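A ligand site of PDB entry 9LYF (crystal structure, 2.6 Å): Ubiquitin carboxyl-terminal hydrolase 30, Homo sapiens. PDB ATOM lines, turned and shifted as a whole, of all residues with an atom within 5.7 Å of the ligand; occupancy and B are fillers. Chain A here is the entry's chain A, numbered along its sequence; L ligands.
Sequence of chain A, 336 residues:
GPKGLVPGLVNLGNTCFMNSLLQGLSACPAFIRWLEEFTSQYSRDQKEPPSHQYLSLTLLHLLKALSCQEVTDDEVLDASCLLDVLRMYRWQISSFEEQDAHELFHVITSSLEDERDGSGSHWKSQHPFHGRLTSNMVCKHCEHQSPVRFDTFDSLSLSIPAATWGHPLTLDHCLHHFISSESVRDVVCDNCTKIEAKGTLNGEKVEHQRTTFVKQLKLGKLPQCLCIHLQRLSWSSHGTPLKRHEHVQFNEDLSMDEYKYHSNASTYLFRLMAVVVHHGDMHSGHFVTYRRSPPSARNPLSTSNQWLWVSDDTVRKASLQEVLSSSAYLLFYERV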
ATOM      1  N   ASN A  11     -11.197 -15.782  -8.128  1.00  0.00           N
ATOM      2  CA  ASN A  11     -11.662 -16.179  -6.794  1.00  0.00           C
ATOM      3  C   ASN A  11     -13.124 -15.786  -6.682  1.00  0.00           C
ATOM      4  O   ASN A  11     -13.440 -14.610  -6.464  1.00  0.00           O
ATOM      5  CB  ASN A  11     -10.818 -15.532  -5.707  1.00  0.00           C
ATOM      6  CG  ASN A  11     -11.078 -16.124  -4.340  1.00  0.00           C
ATOM      7  OD1 ASN A  11     -11.981 -16.943  -4.163  1.00  0.00           O
ATOM      8  ND2 ASN A  11     -10.277 -15.700  -3.356  1.00  0.00           N
ATOM      9  N   GLY A  13     -15.077 -16.437  -4.297  1.00  0.00           N
ATOM     10  CA  GLY A  13     -15.308 -16.007  -2.932  1.00  0.00           C
ATOM     11  C   GLY A  13     -14.551 -16.817  -1.904  1.00  0.00           C
ATOM     12  O   GLY A  13     -14.103 -16.252  -0.900  1.00  0.00           O
ATOM     13  N   ASN A  14     -14.390 -18.124  -2.110  1.00  0.00           N
ATOM     14  CA  ASN A  14     -13.736 -18.886  -1.053  1.00  0.00           C
ATOM     15  C   ASN A  14     -12.643 -19.818  -1.570  1.00  0.00           C
ATOM     16  O   ASN A  14     -12.316 -20.812  -0.905  1.00  0.00           O
ATOM     17  CB  ASN A  14     -14.787 -19.676  -0.240  1.00  0.00           C
ATOM     18  N   THR A  15     -12.049 -19.516  -2.728  1.00  0.00           N
ATOM     19  CA  THR A  15     -10.968 -20.325  -3.255  1.00  0.00           C
ATOM     20  C   THR A  15      -9.657 -19.525  -3.345  1.00  0.00           C
ATOM     21  O   THR A  15      -8.601 -20.047  -3.735  1.00  0.00           O
ATOM     22  CB  THR A  15     -11.343 -20.898  -4.639  1.00  0.00           C
ATOM     23  OG1 THR A  15     -11.438 -19.831  -5.582  1.00  0.00           O
ATOM     24  CG2 THR A  15     -12.667 -21.625  -4.570  1.00  0.00           C
ATOM     25  N   CYS A  16      -9.237 -18.843  -2.149  1.00  0.00           N
ATOM     26  CA  CYS A  16      -7.998 -18.120  -1.974  1.00  0.00           C
ATOM     27  C   CYS A  16      -6.901 -19.033  -1.513  1.00  0.00           C
ATOM     28  O   CYS A  16      -5.759 -18.903  -2.023  1.00  0.00           O
ATOM     29  CB  CYS A  16      -8.120 -16.869  -1.139  1.00  0.00           C
ATOM     30  SG  CYS A  16      -8.784 -17.086   0.550  1.00  0.00           S
ATOM     31  N   PHE A  17      -7.432 -20.055  -0.677  1.00  0.00           N
ATOM     32  CA  PHE A  17      -6.541 -21.022  -0.050  1.00  0.00           C
ATOM     33  C   PHE A  17      -5.899 -21.871  -1.132  1.00  0.00           C
ATOM     34  O   PHE A  17      -4.804 -22.399  -0.976  1.00  0.00           O
ATOM     35  CB  PHE A  17      -7.298 -21.903   0.932  1.00  0.00           C
ATOM     36  CG  PHE A  17      -8.206 -22.877   0.256  1.00  0.00           C
ATOM     37  CD1 PHE A  17      -7.836 -24.195   0.091  1.00  0.00           C
ATOM     38  CD2 PHE A  17      -9.409 -22.450  -0.262  1.00  0.00           C
ATOM     39  CE1 PHE A  17      -8.678 -25.077  -0.564  1.00  0.00           C
ATOM     40  CE2 PHE A  17     -10.249 -23.319  -0.916  1.00  0.00           C
ATOM     41  CZ  PHE A  17      -9.882 -24.636  -1.064  1.00  0.00           C
ATOM     42  N   ASP A 100      -7.733 -23.923   4.485  1.00  0.00           N
ATOM     43  CA  ASP A 100      -6.327 -23.990   4.897  1.00  0.00           C
ATOM     44  C   ASP A 100      -5.388 -24.418   3.776  1.00  0.00           C
ATOM     45  O   ASP A 100      -5.488 -25.538   3.281  1.00  0.00           O
ATOM     46  CB  ASP A 100      -6.148 -24.946   6.081  1.00  0.00           C
ATOM     47  CG  ASP A 100      -4.740 -24.898   6.654  1.00  0.00           C
ATOM     48  OD1 ASP A 100      -3.994 -23.960   6.308  1.00  0.00           O
ATOM     49  OD2 ASP A 100      -4.365 -25.798   7.443  1.00  0.00           O
ATOM     50  N   HIS A 229       6.234 -24.929   7.257  1.00  0.00           N
ATOM     51  CA  HIS A 229       4.934 -24.463   7.712  1.00  0.00           C
ATOM     52  C   HIS A 229       5.066 -23.919   9.130  1.00  0.00           C
ATOM     53  O   HIS A 229       5.601 -24.596  10.013  1.00  0.00           O
ATOM     54  CB  HIS A 229       3.897 -25.587   7.660  1.00  0.00           C
ATOM     55  CG  HIS A 229       2.587 -25.264   8.316  1.00  0.00           C
ATOM     56  ND1 HIS A 229       2.229 -25.758   9.546  1.00  0.00           N
ATOM     57  CD2 HIS A 229       1.530 -24.527   7.888  1.00  0.00           C
ATOM     58  CE1 HIS A 229       1.023 -25.332   9.860  1.00  0.00           C
ATOM     59  NE2 HIS A 229       0.581 -24.581   8.875  1.00  0.00           N
ATOM     60  N   ARG A 232       0.408 -21.265  12.909  1.00  0.00           N
ATOM     61  CA  ARG A 232      -0.233 -20.051  13.392  1.00  0.00           C
ATOM     62  C   ARG A 232      -1.626 -20.301  13.944  1.00  0.00           C
ATOM     63  O   ARG A 232      -2.257 -19.367  14.446  1.00  0.00           O
ATOM     64  CB  ARG A 232      -0.313 -19.007  12.276  1.00  0.00           C
ATOM     65  CG  ARG A 232       1.037 -18.574  11.731  1.00  0.00           C
ATOM     66  CD  ARG A 232       0.923 -17.341  10.846  1.00  0.00           C
ATOM     67  NE  ARG A 232       2.243 -16.912  10.401  1.00  0.00           N
ATOM     68  CZ  ARG A 232       3.063 -16.141  11.107  1.00  0.00           C
ATOM     69  NH1 ARG A 232       2.696 -15.694  12.302  1.00  0.00           N
ATOM     70  NH2 ARG A 232       4.249 -15.816  10.618  1.00  0.00           N
ATOM     71  N   LEU A 233      -2.114 -21.533  13.878  1.00  0.00           N
ATOM     72  CA  LEU A 233      -3.443 -21.883  14.354  1.00  0.00           C
ATOM     73  C   LEU A 233      -3.343 -22.516  15.736  1.00  0.00           C
ATOM     74  O   LEU A 233      -2.727 -23.586  15.884  1.00  0.00           O
ATOM     75  CB  LEU A 233      -4.137 -22.817  13.368  1.00  0.00           C
ATOM     76  CG  LEU A 233      -5.424 -23.458  13.886  1.00  0.00           C
ATOM     77  CD1 LEU A 233      -6.467 -22.403  14.246  1.00  0.00           C
ATOM     78  CD2 LEU A 233      -5.965 -24.424  12.857  1.00  0.00           C
ATOM     79  N   LYS A 243      -5.376 -17.174  16.200  1.00  0.00           N
ATOM     80  CA  LYS A 243      -4.308 -16.934  15.230  1.00  0.00           C
ATOM     81  C   LYS A 243      -3.157 -16.159  15.857  1.00  0.00           C
ATOM     82  O   LYS A 243      -3.373 -15.124  16.504  1.00  0.00           O
ATOM     83  CB  LYS A 243      -4.822 -16.167  14.021  1.00  0.00           C
ATOM     84  CG  LYS A 243      -3.725 -15.931  12.974  1.00  0.00           C
ATOM     85  CD  LYS A 243      -4.232 -15.178  11.760  1.00  0.00           C
ATOM     86  CE  LYS A 243      -3.094 -14.861  10.824  1.00  0.00           C
ATOM     87  NZ  LYS A 243      -3.551 -14.101   9.619  1.00  0.00           N
ATOM     88  N   ARG A 244      -1.939 -16.658  15.658  1.00  0.00           N
ATOM     89  CA  ARG A 244      -0.731 -15.953  16.074  1.00  0.00           C
ATOM     90  C   ARG A 244      -0.250 -15.118  14.899  1.00  0.00           C
ATOM     91  O   ARG A 244       0.091 -15.661  13.837  1.00  0.00           O
ATOM     92  CB  ARG A 244       0.339 -16.920  16.561  1.00  0.00           C
ATOM     93  CG  ARG A 244       0.106 -17.465  17.973  1.00  0.00           C
ATOM     94  CD  ARG A 244       1.390 -17.987  18.588  1.00  0.00           C
ATOM     95  NE  ARG A 244       2.402 -16.946  18.724  1.00  0.00           N
ATOM     96  CZ  ARG A 244       3.622 -17.154  19.223  1.00  0.00           C
ATOM     97  NH1 ARG A 244       3.991 -18.373  19.613  1.00  0.00           N
ATOM     98  NH2 ARG A 244       4.487 -16.152  19.317  1.00  0.00           N
ATOM     99  N   HIS A 278      -1.034 -15.328   5.174  1.00  0.00           N
ATOM    100  CA  HIS A 278      -2.438 -15.256   5.554  1.00  0.00           C
ATOM    101  C   HIS A 278      -2.682 -13.976   6.338  1.00  0.00           C
ATOM    102  O   HIS A 278      -2.028 -13.727   7.359  1.00  0.00           O
ATOM    103  CB  HIS A 278      -2.847 -16.470   6.391  1.00  0.00           C
ATOM    104  CG  HIS A 278      -4.302 -16.470   6.752  1.00  0.00           C
ATOM    105  ND1 HIS A 278      -4.781 -15.918   7.919  1.00  0.00           N
ATOM    106  CD2 HIS A 278      -5.385 -16.919   6.071  1.00  0.00           C
ATOM    107  CE1 HIS A 278      -6.096 -16.048   7.955  1.00  0.00           C
ATOM    108  NE2 HIS A 278      -6.485 -16.656   6.851  1.00  0.00           N
ATOM    109  N   HIS A 279      -3.630 -13.166   5.863  1.00  0.00           N
ATOM    110  CA  HIS A 279      -4.028 -11.931   6.522  1.00  0.00           C
ATOM    111  C   HIS A 279      -5.356 -12.126   7.243  1.00  0.00           C
ATOM    112  O   HIS A 279      -6.049 -13.133   7.066  1.00  0.00           O
ATOM    113  CB  HIS A 279      -4.124 -10.786   5.513  1.00  0.00           C
ATOM    114  CG  HIS A 279      -2.810 -10.356   4.962  1.00  0.00           C
ATOM    115  ND1 HIS A 279      -2.636  -9.932   3.666  1.00  0.00           N
ATOM    116  CD2 HIS A 279      -1.591 -10.294   5.555  1.00  0.00           C
ATOM    117  CE1 HIS A 279      -1.362  -9.619   3.479  1.00  0.00           C
ATOM    118  NE2 HIS A 279      -0.712  -9.825   4.602  1.00  0.00           N
ATOM    119  N   ASP A 281      -8.203 -12.637  10.287  1.00  0.00           N
ATOM    120  CA  ASP A 281      -8.384 -13.629  11.334  1.00  0.00           C
ATOM    121  C   ASP A 281      -8.748 -14.973  10.716  1.00  0.00           C
ATOM    122  O   ASP A 281      -8.747 -15.142   9.484  1.00  0.00           O
ATOM    123  CB  ASP A 281      -9.449 -13.149  12.321  1.00  0.00           C
ATOM    124  CG  ASP A 281     -10.818 -13.016  11.692  1.00  0.00           C
ATOM    125  OD1 ASP A 281     -10.871 -12.794  10.461  1.00  0.00           O
ATOM    126  OD2 ASP A 281     -11.843 -13.118  12.416  1.00  0.00           O
ATOM    127  N   MET A 282      -9.070 -15.941  11.558  1.00  0.00           N
ATOM    128  CA  MET A 282      -9.417 -17.273  11.089  1.00  0.00           C
ATOM    129  C   MET A 282     -10.784 -17.325  10.417  1.00  0.00           C
ATOM    130  O   MET A 282     -11.062 -18.266   9.672  1.00  0.00           O
ATOM    131  CB  MET A 282      -9.365 -18.271  12.253  1.00  0.00           C
ATOM    132  CG  MET A 282      -7.957 -18.480  12.842  1.00  0.00           C
ATOM    133  SD  MET A 282      -6.861 -19.283  11.673  1.00  0.00           S
ATOM    134  CE  MET A 282      -5.274 -19.329  12.501  1.00  0.00           C
ATOM    135  N   HIS A 283     -11.640 -16.328  10.646  1.00  0.00           N
ATOM    136  CA  HIS A 283     -13.014 -16.372  10.143  1.00  0.00           C
ATOM    137  C   HIS A 283     -13.203 -15.571   8.860  1.00  0.00           C
ATOM    138  O   HIS A 283     -13.817 -16.060   7.909  1.00  0.00           O
ATOM    139  CB  HIS A 283     -13.989 -15.882  11.221  1.00  0.00           C
ATOM    140  CG  HIS A 283     -13.841 -16.585  12.536  1.00  0.00           C
ATOM    141  ND1 HIS A 283     -14.349 -17.843  12.759  1.00  0.00           N
ATOM    142  CD2 HIS A 283     -13.241 -16.209  13.692  1.00  0.00           C
ATOM    143  CE1 HIS A 283     -14.076 -18.212  13.996  1.00  0.00           C
ATOM    144  NE2 HIS A 283     -13.403 -17.239  14.579  1.00  0.00           N
ATOM    145  N   SER A 284     -12.694 -14.342   8.807  1.00  0.00           N
ATOM    146  CA  SER A 284     -12.858 -13.466   7.650  1.00  0.00           C
ATOM    147  C   SER A 284     -11.509 -13.040   7.082  1.00  0.00           C
ATOM    148  O   SER A 284     -11.319 -11.894   6.666  1.00  0.00           O
ATOM    149  CB  SER A 284     -13.713 -12.256   8.015  1.00  0.00           C
ATOM    150  OG  SER A 284     -13.059 -11.430   8.967  1.00  0.00           O
ATOM    151  N   GLY A 285     -10.551 -13.957   7.069  1.00  0.00           N
ATOM    152  CA  GLY A 285      -9.224 -13.699   6.564  1.00  0.00           C
ATOM    153  C   GLY A 285      -9.132 -13.757   5.052  1.00  0.00           C
ATOM    154  O   GLY A 285     -10.133 -13.645   4.334  1.00  0.00           O
ATOM    155  N   HIS A 286      -7.910 -13.928   4.572  1.00  0.00           N
ATOM    156  CA  HIS A 286      -7.615 -14.017   3.142  1.00  0.00           C
ATOM    157  C   HIS A 286      -6.197 -14.553   2.972  1.00  0.00           C
ATOM    158  O   HIS A 286      -5.292 -14.220   3.753  1.00  0.00           O
ATOM    159  CB  HIS A 286      -7.756 -12.654   2.449  1.00  0.00           C
ATOM    160  CG  HIS A 286      -7.629 -12.730   0.967  1.00  0.00           C
ATOM    161  ND1 HIS A 286      -8.516 -13.421   0.172  1.00  0.00           N
ATOM    162  CD2 HIS A 286      -6.703 -12.196   0.119  1.00  0.00           C
ATOM    163  CE1 HIS A 286      -8.154 -13.312  -1.098  1.00  0.00           C
ATOM    164  NE2 HIS A 286      -7.058 -12.586  -1.153  1.00  0.00           N
ATOM    165  N   PHE A 287      -6.009 -15.364   1.935  1.00  0.00           N
ATOM    166  CA  PHE A 287      -4.704 -15.922   1.606  1.00  0.00           C
ATOM    167  C   PHE A 287      -4.090 -15.145   0.443  1.00  0.00           C
ATOM    168  O   PHE A 287      -4.791 -14.840  -0.532  1.00  0.00           O
ATOM    169  CB  PHE A 287      -4.808 -17.412   1.264  1.00  0.00           C
ATOM    170  CG  PHE A 287      -4.708 -18.316   2.457  1.00  0.00           C
ATOM    171  CD1 PHE A 287      -3.505 -18.472   3.116  1.00  0.00           C
ATOM    172  CD2 PHE A 287      -5.822 -18.983   2.947  1.00  0.00           C
ATOM    173  CE1 PHE A 287      -3.392 -19.285   4.222  1.00  0.00           C
ATOM    174  CE2 PHE A 287      -5.715 -19.802   4.064  1.00  0.00           C
ATOM    175  CZ  PHE A 287      -4.503 -19.953   4.695  1.00  0.00           C
ATOM    176  N   ASP A 312      -5.041 -13.406  -5.738  1.00  0.00           N
ATOM    177  CA  ASP A 312      -5.952 -13.987  -6.726  1.00  0.00           C
ATOM    178  C   ASP A 312      -5.709 -13.415  -8.125  1.00  0.00           C
ATOM    179  O   ASP A 312      -4.680 -13.699  -8.746  1.00  0.00           O
ATOM    180  CB  ASP A 312      -7.406 -13.775  -6.322  1.00  0.00           C
ATOM    181  CG  ASP A 312      -7.728 -14.423  -5.000  1.00  0.00           C
ATOM    182  OD1 ASP A 312      -7.183 -15.512  -4.741  1.00  0.00           O
ATOM    183  OD2 ASP A 312      -8.500 -13.842  -4.217  1.00  0.00           O
ATOM    184  N   TYR A 329       3.218 -17.745   6.365  1.00  0.00           N
ATOM    185  CA  TYR A 329       2.527 -18.967   6.756  1.00  0.00           C
ATOM    186  C   TYR A 329       3.150 -20.221   6.153  1.00  0.00           C
ATOM    187  O   TYR A 329       3.395 -21.191   6.874  1.00  0.00           O
ATOM    188  CB  TYR A 329       1.039 -18.898   6.360  1.00  0.00           C
ATOM    189  CG  TYR A 329       0.258 -20.139   6.729  1.00  0.00           C
ATOM    190  CD1 TYR A 329       0.107 -20.522   8.064  1.00  0.00           C
ATOM    191  CD2 TYR A 329      -0.349 -20.920   5.750  1.00  0.00           C
ATOM    192  CE1 TYR A 329      -0.607 -21.656   8.408  1.00  0.00           C
ATOM    193  CE2 TYR A 329      -1.076 -22.060   6.092  1.00  0.00           C
ATOM    194  CZ  TYR A 329      -1.195 -22.426   7.419  1.00  0.00           C
ATOM    195  OH  TYR A 329      -1.911 -23.553   7.757  1.00  0.00           O
HETATM  196  C1  LIG L   1     -10.200 -18.077   6.407  1.00  0.00           C
HETATM  197  C2  LIG L   1     -12.317 -17.178   5.197  1.00  0.00           C
HETATM  198  C3  LIG L   1     -11.737 -16.254   4.090  1.00  0.00           C
HETATM  199  C4  LIG L   1     -12.737 -15.715   3.412  1.00  0.00           C
HETATM  200  C5  LIG L   1     -12.742 -16.474   1.937  1.00  0.00           C
HETATM  201  C6  LIG L   1     -10.611 -16.615   0.487  1.00  0.00           C
HETATM  202  C7  LIG L   1     -10.902 -17.191   3.061  1.00  0.00           C
HETATM  203  C8  LIG L   1      -9.334 -19.226   6.816  1.00  0.00           C
HETATM  204  C9  LIG L   1      -7.699 -20.381   7.690  1.00  0.00           C
HETATM  205  C10 LIG L   1      -6.366 -20.745   8.393  1.00  0.00           C
HETATM  206  C11 LIG L   1      -5.382 -19.793   8.561  1.00  0.00           C
HETATM  207  C12 LIG L   1      -4.186 -20.134   9.181  1.00  0.00           C
HETATM  208  C13 LIG L   1      -3.049 -19.065   9.385  1.00  0.00           C
HETATM  209  C14 LIG L   1      -3.988 -21.411   9.625  1.00  0.00           C
HETATM  210  C15 LIG L   1      -4.985 -22.369   9.455  1.00  0.00           C
HETATM  211  C16 LIG L   1      -6.169 -22.036   8.836  1.00  0.00           C
HETATM  212  N1  LIG L   1     -11.408 -18.318   5.555  1.00  0.00           N
HETATM  213  N2  LIG L   1     -11.443 -16.747   1.736  1.00  0.00           N
HETATM  214  N3  LIG L   1     -11.130 -16.231  -0.616  1.00  0.00           N
HETATM  215  N4  LIG L   1      -9.620 -20.509   6.650  1.00  0.00           N
HETATM  216  N5  LIG L   1      -8.585 -21.237   7.191  1.00  0.00           N
HETATM  217  N6  LIG L   1      -2.226 -18.293   9.541  1.00  0.00           N
HETATM  218  O1  LIG L   1      -9.962 -16.995   6.779  1.00  0.00           O
HETATM  219  O2  LIG L   1      -8.166 -19.158   7.465  1.00  0.00           O
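The side-chain sulfur of Cys 16 is bonded to a carbon (C6) of the ligand (1.9 Å).
The side-chain amide nitrogen (ND2) of Asn 11 lies close to a nitrogen (N3) of the ligand (2.9 Å).
The backbone carbonyl oxygen of Gly 13 lies within hydrogen-bond range of a nitrogen (N3) of the ligand (3.0 Å).
An oxygen (O1) of the ligand lies within hydrogen-bond range of the backbone NH (N) of Gly 285, at 3.1 Å.
NE2 of His 278 lies within hydrogen-bond range of O2 of the ligand (3.1 Å).
The side-chain sulfur (SG) of Cys 16 lies within hydrogen-bond range of a ring nitrogen (ND1) of His 286 (3.7 Å).
OD1 of Asn 11 sits at hydrogen-bond distance from N of Gly 13.
OD1 of Asn 11 is in hydrogen-bond range of N of Thr 15 (2.9 Å).
The backbone carbonyl oxygen of His 278 lies within hydrogen-bond range of the side-chain amino group of Lys 243, 2.8 Å away.
The backbone carbonyl oxygen (O) of Arg 232 lies within hydrogen-bond range of the backbone NH (N) of Arg 244, 3.0 Å away.
The side-chain hydroxyl of Tyr 329 lies within hydrogen-bond range of the side-chain carboxylate of Asp 100, at 2.6 Å.
NE2 of His 229 sits at hydrogen-bond distance from OH of Tyr 329 (2.9 Å).
O of His 286 is in hydrogen-bond range of N of His 279.
The backbone carbonyl oxygen of Asp 281 lies close to an oxygen (O1) of the ligand (3.5 Å).
An oxygen (O1) of the ligand sits close to the backbone carbonyl oxygen (O) of Met 282 (3.3 Å).
Residues that only touch the ligand: Asn 14 (3.7 Å), Asp 100 (3.7 Å), Arg 232 (3.4 Å), Lys 243 (3.8 Å), His 283 (3.3 Å), His 286 (3.8 Å), Phe 287 (3.97 Å) and Tyr 329 (3.5 Å).
The nearest printed residue that does not touch the ligand is Leu 233 (4.001 Å).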
